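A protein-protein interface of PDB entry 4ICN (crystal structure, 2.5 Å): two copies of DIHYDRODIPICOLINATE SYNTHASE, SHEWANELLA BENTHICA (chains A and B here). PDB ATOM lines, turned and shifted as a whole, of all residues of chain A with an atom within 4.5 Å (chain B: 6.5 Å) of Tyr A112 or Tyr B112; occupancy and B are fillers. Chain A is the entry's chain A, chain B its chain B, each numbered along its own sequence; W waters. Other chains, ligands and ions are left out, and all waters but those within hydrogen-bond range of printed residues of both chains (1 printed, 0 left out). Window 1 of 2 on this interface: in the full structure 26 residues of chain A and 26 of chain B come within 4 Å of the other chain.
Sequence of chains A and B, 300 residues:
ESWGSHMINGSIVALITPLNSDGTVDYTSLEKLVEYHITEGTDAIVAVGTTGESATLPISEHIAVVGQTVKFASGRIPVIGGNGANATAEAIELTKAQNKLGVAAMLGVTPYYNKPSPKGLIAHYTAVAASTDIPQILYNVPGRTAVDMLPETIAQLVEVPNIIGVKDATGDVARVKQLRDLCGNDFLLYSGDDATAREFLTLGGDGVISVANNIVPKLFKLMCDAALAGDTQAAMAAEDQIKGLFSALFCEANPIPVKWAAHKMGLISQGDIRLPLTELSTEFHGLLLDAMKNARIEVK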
ATOM      1  N   GLY A  84      29.906 -22.110 -29.560  1.00  0.00           N
ATOM      2  CA  GLY A  84      30.497 -21.772 -28.260  1.00  0.00           C
ATOM      3  C   GLY A  84      29.465 -21.827 -27.152  1.00  0.00           C
ATOM      4  O   GLY A  84      28.304 -21.475 -27.377  1.00  0.00           O
ATOM      5  N   ALA A  85      29.866 -22.288 -25.972  1.00  0.00           N
ATOM      6  CA  ALA A  85      28.976 -22.306 -24.806  1.00  0.00           C
ATOM      7  C   ALA A  85      29.797 -22.456 -23.521  1.00  0.00           C
ATOM      8  O   ALA A  85      30.853 -23.041 -23.545  1.00  0.00           O
ATOM      9  CB  ALA A  85      27.966 -23.434 -24.915  1.00  0.00           C
ATOM     10  N   ASN A  86      29.304 -21.938 -22.398  1.00  0.00           N
ATOM     11  CA  ASN A  86      30.017 -22.092 -21.148  1.00  0.00           C
ATOM     12  C   ASN A  86      29.634 -23.335 -20.330  1.00  0.00           C
ATOM     13  O   ASN A  86      30.177 -23.592 -19.254  1.00  0.00           O
ATOM     14  CB  ASN A  86      29.974 -20.794 -20.348  1.00  0.00           C
ATOM     15  CG  ASN A  86      28.589 -20.419 -19.893  1.00  0.00           C
ATOM     16  OD1 ASN A  86      27.613 -21.058 -20.250  1.00  0.00           O
ATOM     17  ND2 ASN A  86      28.501 -19.381 -19.079  1.00  0.00           N
ATOM     18  N   VAL A 109      34.201 -20.465 -28.835  1.00  0.00           N
ATOM     19  CA  VAL A 109      34.815 -19.738 -27.714  1.00  0.00           C
ATOM     20  C   VAL A 109      34.981 -20.610 -26.463  1.00  0.00           C
ATOM     21  O   VAL A 109      34.174 -21.484 -26.194  1.00  0.00           O
ATOM     22  CB  VAL A 109      34.041 -18.426 -27.409  1.00  0.00           C
ATOM     23  CG1 VAL A 109      32.687 -18.709 -26.811  1.00  0.00           C
ATOM     24  CG2 VAL A 109      34.844 -17.516 -26.530  1.00  0.00           C
ATOM     25  N   THR A 110      36.061 -20.387 -25.732  1.00  0.00           N
ATOM     26  CA  THR A 110      36.245 -20.993 -24.408  1.00  0.00           C
ATOM     27  C   THR A 110      35.074 -20.574 -23.520  1.00  0.00           C
ATOM     28  O   THR A 110      34.619 -19.427 -23.614  1.00  0.00           O
ATOM     29  CB  THR A 110      37.462 -20.383 -23.716  1.00  0.00           C
ATOM     30  OG1 THR A 110      37.202 -18.986 -23.560  1.00  0.00           O
ATOM     31  CG2 THR A 110      38.714 -20.526 -24.556  1.00  0.00           C
ATOM     32  N   PRO A 111      34.593 -21.484 -22.650  1.00  0.00           N
ATOM     33  CA  PRO A 111      33.611 -21.176 -21.623  1.00  0.00           C
ATOM     34  C   PRO A 111      33.847 -19.840 -20.945  1.00  0.00           C
ATOM     35  O   PRO A 111      34.944 -19.567 -20.479  1.00  0.00           O
ATOM     36  CB  PRO A 111      33.828 -22.303 -20.627  1.00  0.00           C
ATOM     37  CG  PRO A 111      34.077 -23.455 -21.530  1.00  0.00           C
ATOM     38  CD  PRO A 111      34.944 -22.914 -22.627  1.00  0.00           C
ATOM     39  N   TYR A 112      32.808 -19.016 -20.889  1.00  0.00           N
ATOM     40  CA  TYR A 112      32.918 -17.669 -20.335  1.00  0.00           C
ATOM     41  C   TYR A 112      32.201 -17.575 -19.021  1.00  0.00           C
ATOM     42  O   TYR A 112      31.402 -18.441 -18.657  1.00  0.00           O
ATOM     43  CB  TYR A 112      32.328 -16.636 -21.292  1.00  0.00           C
ATOM     44  CG  TYR A 112      31.102 -17.133 -22.005  1.00  0.00           C
ATOM     45  CD1 TYR A 112      29.836 -16.936 -21.473  1.00  0.00           C
ATOM     46  CD2 TYR A 112      31.224 -17.840 -23.213  1.00  0.00           C
ATOM     47  CE1 TYR A 112      28.720 -17.409 -22.119  1.00  0.00           C
ATOM     48  CE2 TYR A 112      30.116 -18.315 -23.883  1.00  0.00           C
ATOM     49  CZ  TYR A 112      28.859 -18.099 -23.335  1.00  0.00           C
ATOM     50  OH  TYR A 112      27.756 -18.596 -24.012  1.00  0.00           O
ATOM     51  N   TYR A 113      32.513 -16.517 -18.297  1.00  0.00           N
ATOM     52  CA  TYR A 113      31.924 -16.263 -16.993  1.00  0.00           C
ATOM     53  C   TYR A 113      32.282 -17.265 -15.890  1.00  0.00           C
ATOM     54  O   TYR A 113      32.549 -16.843 -14.788  1.00  0.00           O
ATOM     55  CB  TYR A 113      30.403 -16.066 -17.107  1.00  0.00           C
ATOM     56  CG  TYR A 113      29.715 -15.789 -15.813  1.00  0.00           C
ATOM     57  CD1 TYR A 113      29.759 -14.519 -15.233  1.00  0.00           C
ATOM     58  CD2 TYR A 113      29.007 -16.793 -15.155  1.00  0.00           C
ATOM     59  CE1 TYR A 113      29.117 -14.256 -14.042  1.00  0.00           C
ATOM     60  CE2 TYR A 113      28.354 -16.539 -13.949  1.00  0.00           C
ATOM     61  CZ  TYR A 113      28.416 -15.264 -13.408  1.00  0.00           C
ATOM     62  OH  TYR A 113      27.774 -15.013 -12.215  1.00  0.00           O
ATOM     63  N   ASN A 114      32.246 -18.565 -16.147  1.00  0.00           N
ATOM     64  CA  ASN A 114      32.453 -19.539 -15.033  1.00  0.00           C
ATOM     65  C   ASN A 114      33.929 -19.894 -14.777  1.00  0.00           C
ATOM     66  O   ASN A 114      34.247 -20.546 -13.801  1.00  0.00           O
ATOM     67  CB  ASN A 114      31.573 -20.799 -15.156  1.00  0.00           C
ATOM     68  CG  ASN A 114      31.691 -21.443 -16.514  1.00  0.00           C
ATOM     69  OD1 ASN A 114      32.425 -20.949 -17.399  1.00  0.00           O
ATOM     70  ND2 ASN A 114      30.945 -22.519 -16.722  1.00  0.00           N
ATOM     71  N   THR A 145      35.944 -13.320 -21.840  1.00  0.00           N
ATOM     72  CA  THR A 145      35.570 -14.569 -21.200  1.00  0.00           C
ATOM     73  C   THR A 145      36.091 -14.639 -19.787  1.00  0.00           C
ATOM     74  O   THR A 145      35.573 -15.402 -18.965  1.00  0.00           O
ATOM     75  CB  THR A 145      36.163 -15.776 -21.961  1.00  0.00           C
ATOM     76  OG1 THR A 145      37.600 -15.751 -21.854  1.00  0.00           O
ATOM     77  CG2 THR A 145      35.734 -15.743 -23.426  1.00  0.00           C
ATOM     78  N   SER B  54      25.007 -21.777 -11.809  1.00  0.00           N
ATOM     79  CA  SER B  54      23.963 -21.399 -12.774  1.00  0.00           C
ATOM     80  C   SER B  54      24.331 -21.605 -14.256  1.00  0.00           C
ATOM     81  O   SER B  54      23.475 -21.927 -15.086  1.00  0.00           O
ATOM     82  CB  SER B  54      23.506 -19.946 -12.557  1.00  0.00           C
ATOM     83  OG  SER B  54      24.602 -19.040 -12.642  1.00  0.00           O
ATOM     84  N   ALA B  55      25.599 -21.414 -14.586  1.00  0.00           N
ATOM     85  CA  ALA B  55      26.073 -21.581 -15.959  1.00  0.00           C
ATOM     86  C   ALA B  55      25.724 -22.951 -16.546  1.00  0.00           C
ATOM     87  O   ALA B  55      25.420 -23.071 -17.738  1.00  0.00           O
ATOM     88  CB  ALA B  55      27.558 -21.366 -16.017  1.00  0.00           C
ATOM     89  N   GLY B  84      19.982 -14.322 -13.620  1.00  0.00           N
ATOM     90  CA  GLY B  84      20.894 -13.614 -14.538  1.00  0.00           C
ATOM     91  C   GLY B  84      20.990 -14.301 -15.889  1.00  0.00           C
ATOM     92  O   GLY B  84      20.960 -15.539 -15.979  1.00  0.00           O
ATOM     93  N   ALA B  85      21.100 -13.518 -16.947  1.00  0.00           N
ATOM     94  CA  ALA B  85      21.433 -14.072 -18.256  1.00  0.00           C
ATOM     95  C   ALA B  85      22.026 -12.958 -19.057  1.00  0.00           C
ATOM     96  O   ALA B  85      21.867 -11.794 -18.699  1.00  0.00           O
ATOM     97  CB  ALA B  85      20.210 -14.590 -18.955  1.00  0.00           C
ATOM     98  N   ASN B  86      22.703 -13.284 -20.145  1.00  0.00           N
ATOM     99  CA  ASN B  86      23.280 -12.235 -20.961  1.00  0.00           C
ATOM    100  C   ASN B  86      22.421 -11.874 -22.181  1.00  0.00           C
ATOM    101  O   ASN B  86      22.787 -11.029 -22.981  1.00  0.00           O
ATOM    102  CB  ASN B  86      24.734 -12.536 -21.310  1.00  0.00           C
ATOM    103  CG  ASN B  86      24.885 -13.750 -22.197  1.00  0.00           C
ATOM    104  OD1 ASN B  86      23.942 -14.479 -22.411  1.00  0.00           O
ATOM    105  ND2 ASN B  86      26.082 -13.964 -22.717  1.00  0.00           N
ATOM    106  N   GLU B  90      16.210 -13.955 -22.520  1.00  0.00           N
ATOM    107  CA  GLU B  90      16.449 -15.149 -21.684  1.00  0.00           C
ATOM    108  C   GLU B  90      16.240 -14.839 -20.212  1.00  0.00           C
ATOM    109  O   GLU B  90      15.662 -15.640 -19.478  1.00  0.00           O
ATOM    110  CB  GLU B  90      17.856 -15.730 -21.932  1.00  0.00           C
ATOM    111  CG  GLU B  90      18.186 -17.124 -21.312  1.00  0.00           C
ATOM    112  CD  GLU B  90      19.698 -17.525 -21.461  1.00  0.00           C
ATOM    113  OE1 GLU B  90      20.534 -16.685 -21.908  1.00  0.00           O
ATOM    114  OE2 GLU B  90      20.058 -18.686 -21.124  1.00  0.00           O
ATOM    115  N   VAL B 109      22.814 -11.207 -12.221  1.00  0.00           N
ATOM    116  CA  VAL B 109      24.119 -10.756 -12.652  1.00  0.00           C
ATOM    117  C   VAL B 109      24.003  -9.935 -13.925  1.00  0.00           C
ATOM    118  O   VAL B 109      23.099 -10.154 -14.721  1.00  0.00           O
ATOM    119  CB  VAL B 109      25.123 -11.964 -12.791  1.00  0.00           C
ATOM    120  CG1 VAL B 109      24.871 -12.785 -14.064  1.00  0.00           C
ATOM    121  CG2 VAL B 109      26.524 -11.470 -12.799  1.00  0.00           C
ATOM    122  N   THR B 110      24.888  -8.958 -14.091  1.00  0.00           N
ATOM    123  CA  THR B 110      24.962  -8.153 -15.331  1.00  0.00           C
ATOM    124  C   THR B 110      25.327  -9.065 -16.517  1.00  0.00           C
ATOM    125  O   THR B 110      26.067 -10.048 -16.330  1.00  0.00           O
ATOM    126  CB  THR B 110      26.072  -7.064 -15.235  1.00  0.00           C
ATOM    127  OG1 THR B 110      27.361  -7.702 -15.148  1.00  0.00           O
ATOM    128  CG2 THR B 110      25.884  -6.184 -14.006  1.00  0.00           C
ATOM    129  N   PRO B 111      24.817  -8.759 -17.724  1.00  0.00           N
ATOM    130  CA  PRO B 111      25.145  -9.601 -18.860  1.00  0.00           C
ATOM    131  C   PRO B 111      26.656  -9.774 -19.069  1.00  0.00           C
ATOM    132  O   PRO B 111      27.402  -8.802 -19.159  1.00  0.00           O
ATOM    133  CB  PRO B 111      24.492  -8.857 -20.025  1.00  0.00           C
ATOM    134  CG  PRO B 111      23.277  -8.245 -19.406  1.00  0.00           C
ATOM    135  CD  PRO B 111      23.753  -7.790 -18.055  1.00  0.00           C
ATOM    136  N   TYR B 112      27.105 -11.024 -19.117  1.00  0.00           N
ATOM    137  CA  TYR B 112      28.526 -11.323 -19.245  1.00  0.00           C
ATOM    138  C   TYR B 112      28.850 -11.632 -20.683  1.00  0.00           C
ATOM    139  O   TYR B 112      27.942 -11.879 -21.490  1.00  0.00           O
ATOM    140  CB  TYR B 112      28.888 -12.501 -18.371  1.00  0.00           C
ATOM    141  CG  TYR B 112      27.830 -13.530 -18.375  1.00  0.00           C
ATOM    142  CD1 TYR B 112      27.716 -14.453 -19.423  1.00  0.00           C
ATOM    143  CD2 TYR B 112      26.917 -13.580 -17.345  1.00  0.00           C
ATOM    144  CE1 TYR B 112      26.705 -15.401 -19.424  1.00  0.00           C
ATOM    145  CE2 TYR B 112      25.911 -14.505 -17.331  1.00  0.00           C
ATOM    146  CZ  TYR B 112      25.798 -15.422 -18.365  1.00  0.00           C
ATOM    147  OH  TYR B 112      24.770 -16.345 -18.298  1.00  0.00           O
ATOM    148  N   TYR B 113      30.139 -11.579 -20.999  1.00  0.00           N
ATOM    149  CA  TYR B 113      30.656 -11.870 -22.334  1.00  0.00           C
ATOM    150  C   TYR B 113      30.352 -10.834 -23.448  1.00  0.00           C
ATOM    151  O   TYR B 113      31.256 -10.466 -24.207  1.00  0.00           O
ATOM    152  CB  TYR B 113      30.262 -13.288 -22.781  1.00  0.00           C
ATOM    153  CG  TYR B 113      30.859 -13.682 -24.094  1.00  0.00           C
ATOM    154  CD1 TYR B 113      32.218 -13.983 -24.197  1.00  0.00           C
ATOM    155  CD2 TYR B 113      30.079 -13.755 -25.241  1.00  0.00           C
ATOM    156  CE1 TYR B 113      32.790 -14.329 -25.417  1.00  0.00           C
ATOM    157  CE2 TYR B 113      30.629 -14.138 -26.462  1.00  0.00           C
ATOM    158  CZ  TYR B 113      31.991 -14.418 -26.538  1.00  0.00           C
ATOM    159  OH  TYR B 113      32.552 -14.773 -27.743  1.00  0.00           O
ATOM    160  N   ASN B 114      29.105 -10.383 -23.566  1.00  0.00           N
ATOM    161  CA  ASN B 114      28.745  -9.504 -24.707  1.00  0.00           C
ATOM    162  C   ASN B 114      29.004  -7.975 -24.502  1.00  0.00           C
ATOM    163  O   ASN B 114      28.902  -7.190 -25.439  1.00  0.00           O
ATOM    164  CB  ASN B 114      27.341  -9.813 -25.261  1.00  0.00           C
ATOM    165  CG  ASN B 114      26.235  -9.789 -24.179  1.00  0.00           C
ATOM    166  OD1 ASN B 114      26.489  -9.586 -22.998  1.00  0.00           O
ATOM    167  ND2 ASN B 114      25.016 -10.025 -24.593  1.00  0.00           N
ATOM    168  N   LYS B 115      29.395  -7.584 -23.291  1.00  0.00           N
ATOM    169  CA  LYS B 115      29.824  -6.199 -22.983  1.00  0.00           C
ATOM    170  C   LYS B 115      28.866  -5.097 -23.462  1.00  0.00           C
ATOM    171  O   LYS B 115      29.245  -4.237 -24.236  1.00  0.00           O
ATOM    172  CB  LYS B 115      31.231  -5.919 -23.499  1.00  0.00           C
ATOM    173  CG  LYS B 115      32.301  -6.666 -22.749  1.00  0.00           C
ATOM    174  CD  LYS B 115      33.685  -6.446 -23.344  1.00  0.00           C
ATOM    175  CE  LYS B 115      34.049  -4.958 -23.482  1.00  0.00           C
ATOM    176  NZ  LYS B 115      35.540  -4.839 -23.698  1.00  0.00           N
ATOM    177  N   PRO B 116      27.623  -5.118 -22.982  1.00  0.00           N
ATOM    178  CA  PRO B 116      26.719  -4.052 -23.347  1.00  0.00           C
ATOM    179  C   PRO B 116      27.162  -2.721 -22.735  1.00  0.00           C
ATOM    180  O   PRO B 116      27.926  -2.694 -21.779  1.00  0.00           O
ATOM    181  CB  PRO B 116      25.399  -4.499 -22.713  1.00  0.00           C
ATOM    182  CG  PRO B 116      25.810  -5.276 -21.543  1.00  0.00           C
ATOM    183  CD  PRO B 116      27.089  -5.959 -21.891  1.00  0.00           C
ATOM    184  N   ARG B 144      34.320 -11.397 -13.697  1.00  0.00           N
ATOM    185  CA  ARG B 144      33.713 -12.508 -14.410  1.00  0.00           C
ATOM    186  C   ARG B 144      32.938 -12.142 -15.667  1.00  0.00           C
ATOM    187  O   ARG B 144      32.804 -12.970 -16.557  1.00  0.00           O
ATOM    188  CB  ARG B 144      32.809 -13.293 -13.466  1.00  0.00           C
ATOM    189  CG  ARG B 144      33.589 -14.244 -12.571  1.00  0.00           C
ATOM    190  CD  ARG B 144      32.621 -14.864 -11.617  1.00  0.00           C
ATOM    191  NE  ARG B 144      33.259 -15.826 -10.707  1.00  0.00           N
ATOM    192  CZ  ARG B 144      33.457 -17.107 -10.989  1.00  0.00           C
ATOM    193  NH1 ARG B 144      33.095 -17.591 -12.175  1.00  0.00           N
ATOM    194  NH2 ARG B 144      34.024 -17.888 -10.077  1.00  0.00           N
ATOM    195  N   THR B 145      32.457 -10.909 -15.758  1.00  0.00           N
ATOM    196  CA  THR B 145      31.504 -10.551 -16.793  1.00  0.00           C
ATOM    197  C   THR B 145      32.106  -9.730 -17.888  1.00  0.00           C
ATOM    198  O   THR B 145      31.469  -9.518 -18.926  1.00  0.00           O
ATOM    199  CB  THR B 145      30.363  -9.664 -16.215  1.00  0.00           C
ATOM    200  OG1 THR B 145      30.901  -8.407 -15.803  1.00  0.00           O
ATOM    201  CG2 THR B 145      29.615 -10.359 -15.053  1.00  0.00           C
ATOM    202  N   ALA B 146      33.306  -9.208 -17.635  1.00  0.00           N
ATOM    203  CA  ALA B 146      33.931  -8.216 -18.525  1.00  0.00           C
ATOM    204  C   ALA B 146      33.200  -6.866 -18.588  1.00  0.00           C
ATOM    205  O   ALA B 146      33.495  -6.041 -19.440  1.00  0.00           O
ATOM    206  CB  ALA B 146      34.128  -8.780 -19.938  1.00  0.00           C
ATOM    207  N   VAL B 147      32.256  -6.619 -17.695  1.00  0.00           N
ATOM    208  CA  VAL B 147      31.641  -5.296 -17.669  1.00  0.00           C
ATOM    209  C   VAL B 147      31.519  -4.753 -16.255  1.00  0.00           C
ATOM    210  O   VAL B 147      31.079  -5.448 -15.371  1.00  0.00           O
ATOM    211  CB  VAL B 147      30.267  -5.284 -18.403  1.00  0.00           C
ATOM    212  CG1 VAL B 147      29.240  -6.186 -17.684  1.00  0.00           C
ATOM    213  CG2 VAL B 147      29.756  -3.871 -18.548  1.00  0.00           C
HETATM  214  O   HOH W   1      32.071 -13.371 -19.231  1.00  0.00           O
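The backbone carbonyl oxygen (O) of Tyr A113 is in hydrogen-bond range of the guanidinium group (NH1) of Arg B144 (2.8 Å).
The backbone carbonyl oxygen (O) of Tyr A112 lies close to the side-chain amide oxygen (OD1) of Asn A114, at 3.0 Å. The backbone carbonyl oxygen of Tyr B112 sits at hydrogen-bond distance from the side-chain amide nitrogen of Asn B86. The backbone carbonyl oxygen (O) of Tyr B112 lies close to the side-chain amide oxygen (OD1) of Asn B114 (3.1 Å). The backbone carbonyl oxygen (O) of Thr B145 sits at hydrogen-bond distance from the backbone NH (N) of Tyr B113, 3.2 Å away. The side-chain amide nitrogen (ND2) of Asn A114 lies within hydrogen-bond range of the backbone carbonyl oxygen (O) of Asn A86 (2.9 Å). The backbone carbonyl oxygen (O) of Tyr A112 is in hydrogen-bond range of the side-chain amide nitrogen (ND2) of Asn A86.
Asn A86 touches Ala B55 (ND2 to CB, 3.8 Å). Tyr B113 touches Val A109 (OH to CG2, 3.8 Å). Tyr B112 touches Tyr A112. Tyr B113 touches Tyr A112. Tyr A113 touches Val B109. Tyr A113 touches Tyr B112 (CD1 to CD2, 3.7 Å). CB of Ala B55 touches ND2 of Asn A114 (3.6 Å). Arg B144 touches Asn A114 (NH1 to CA, 3.5 Å). Thr A145 touches Tyr B113.
Of the printed residues of chain B, Tyr A112 touches Tyr B112 and Tyr B113. Of chain A, only Tyr A112 and Tyr A113 come within 4 Å of Tyr B112. Of the printed residues of chain A, Ala B55 touches Asn A86 (3.8 Å) and Asn A114 (3.6 Å). Of the printed residues of chain B, Tyr A113 touches Val B109, Tyr B112 and Arg B144. Printed residues of chain A within 4 Å of Val B109: Tyr A113 (3.8 Å). Of the printed residues of chain B, Val A109 touches Tyr B113. Of the printed residues of chain A, Tyr B113 touches Val A109 (3.8 Å), Tyr A112 (3.9 Å) and Thr A145 (3.8 Å). Thr B145 touches none of the printed residues of chain A. The nearest printed residue of chain B that does not touch Tyr A113 is Thr B145 (4.1 Å).
Of the 18 printed residues of chain B, 5 touch a printed residue of chain A. Printed residues of chain B that touch a printed residue of chain A: Ala B55, Val B109, Tyr B112, Tyr B113 and Arg B144. Hydrophobic or aromatic side chains of chain A within 4 Å of the printed part of chain B: Val A109, Tyr A112 and Tyr A113. Among the printed residues, 10 pairs touch across the chains.
Val A109 touches Tyr B113, and with the chains exchanged Tyr A113 touches Val B109. Tyr A112 touches its own counterpart, Tyr B112. Tyr A112 touches Tyr B113, and with the chains exchanged Tyr A113 touches Tyr B112. Thr A145 touches Tyr B113, but with the chains exchanged Tyr A113 does not touch Thr B145 (4.1 Å). Positions printed for both chains: 84, 85, 86, 109, 110, 111, 112, 113, 114 and 145.
Water W1 lies within hydrogen-bond range of the backbone carbonyl oxygen of Arg B144, the backbone NH of Tyr B113 and the backbone NH of Tyr A113.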
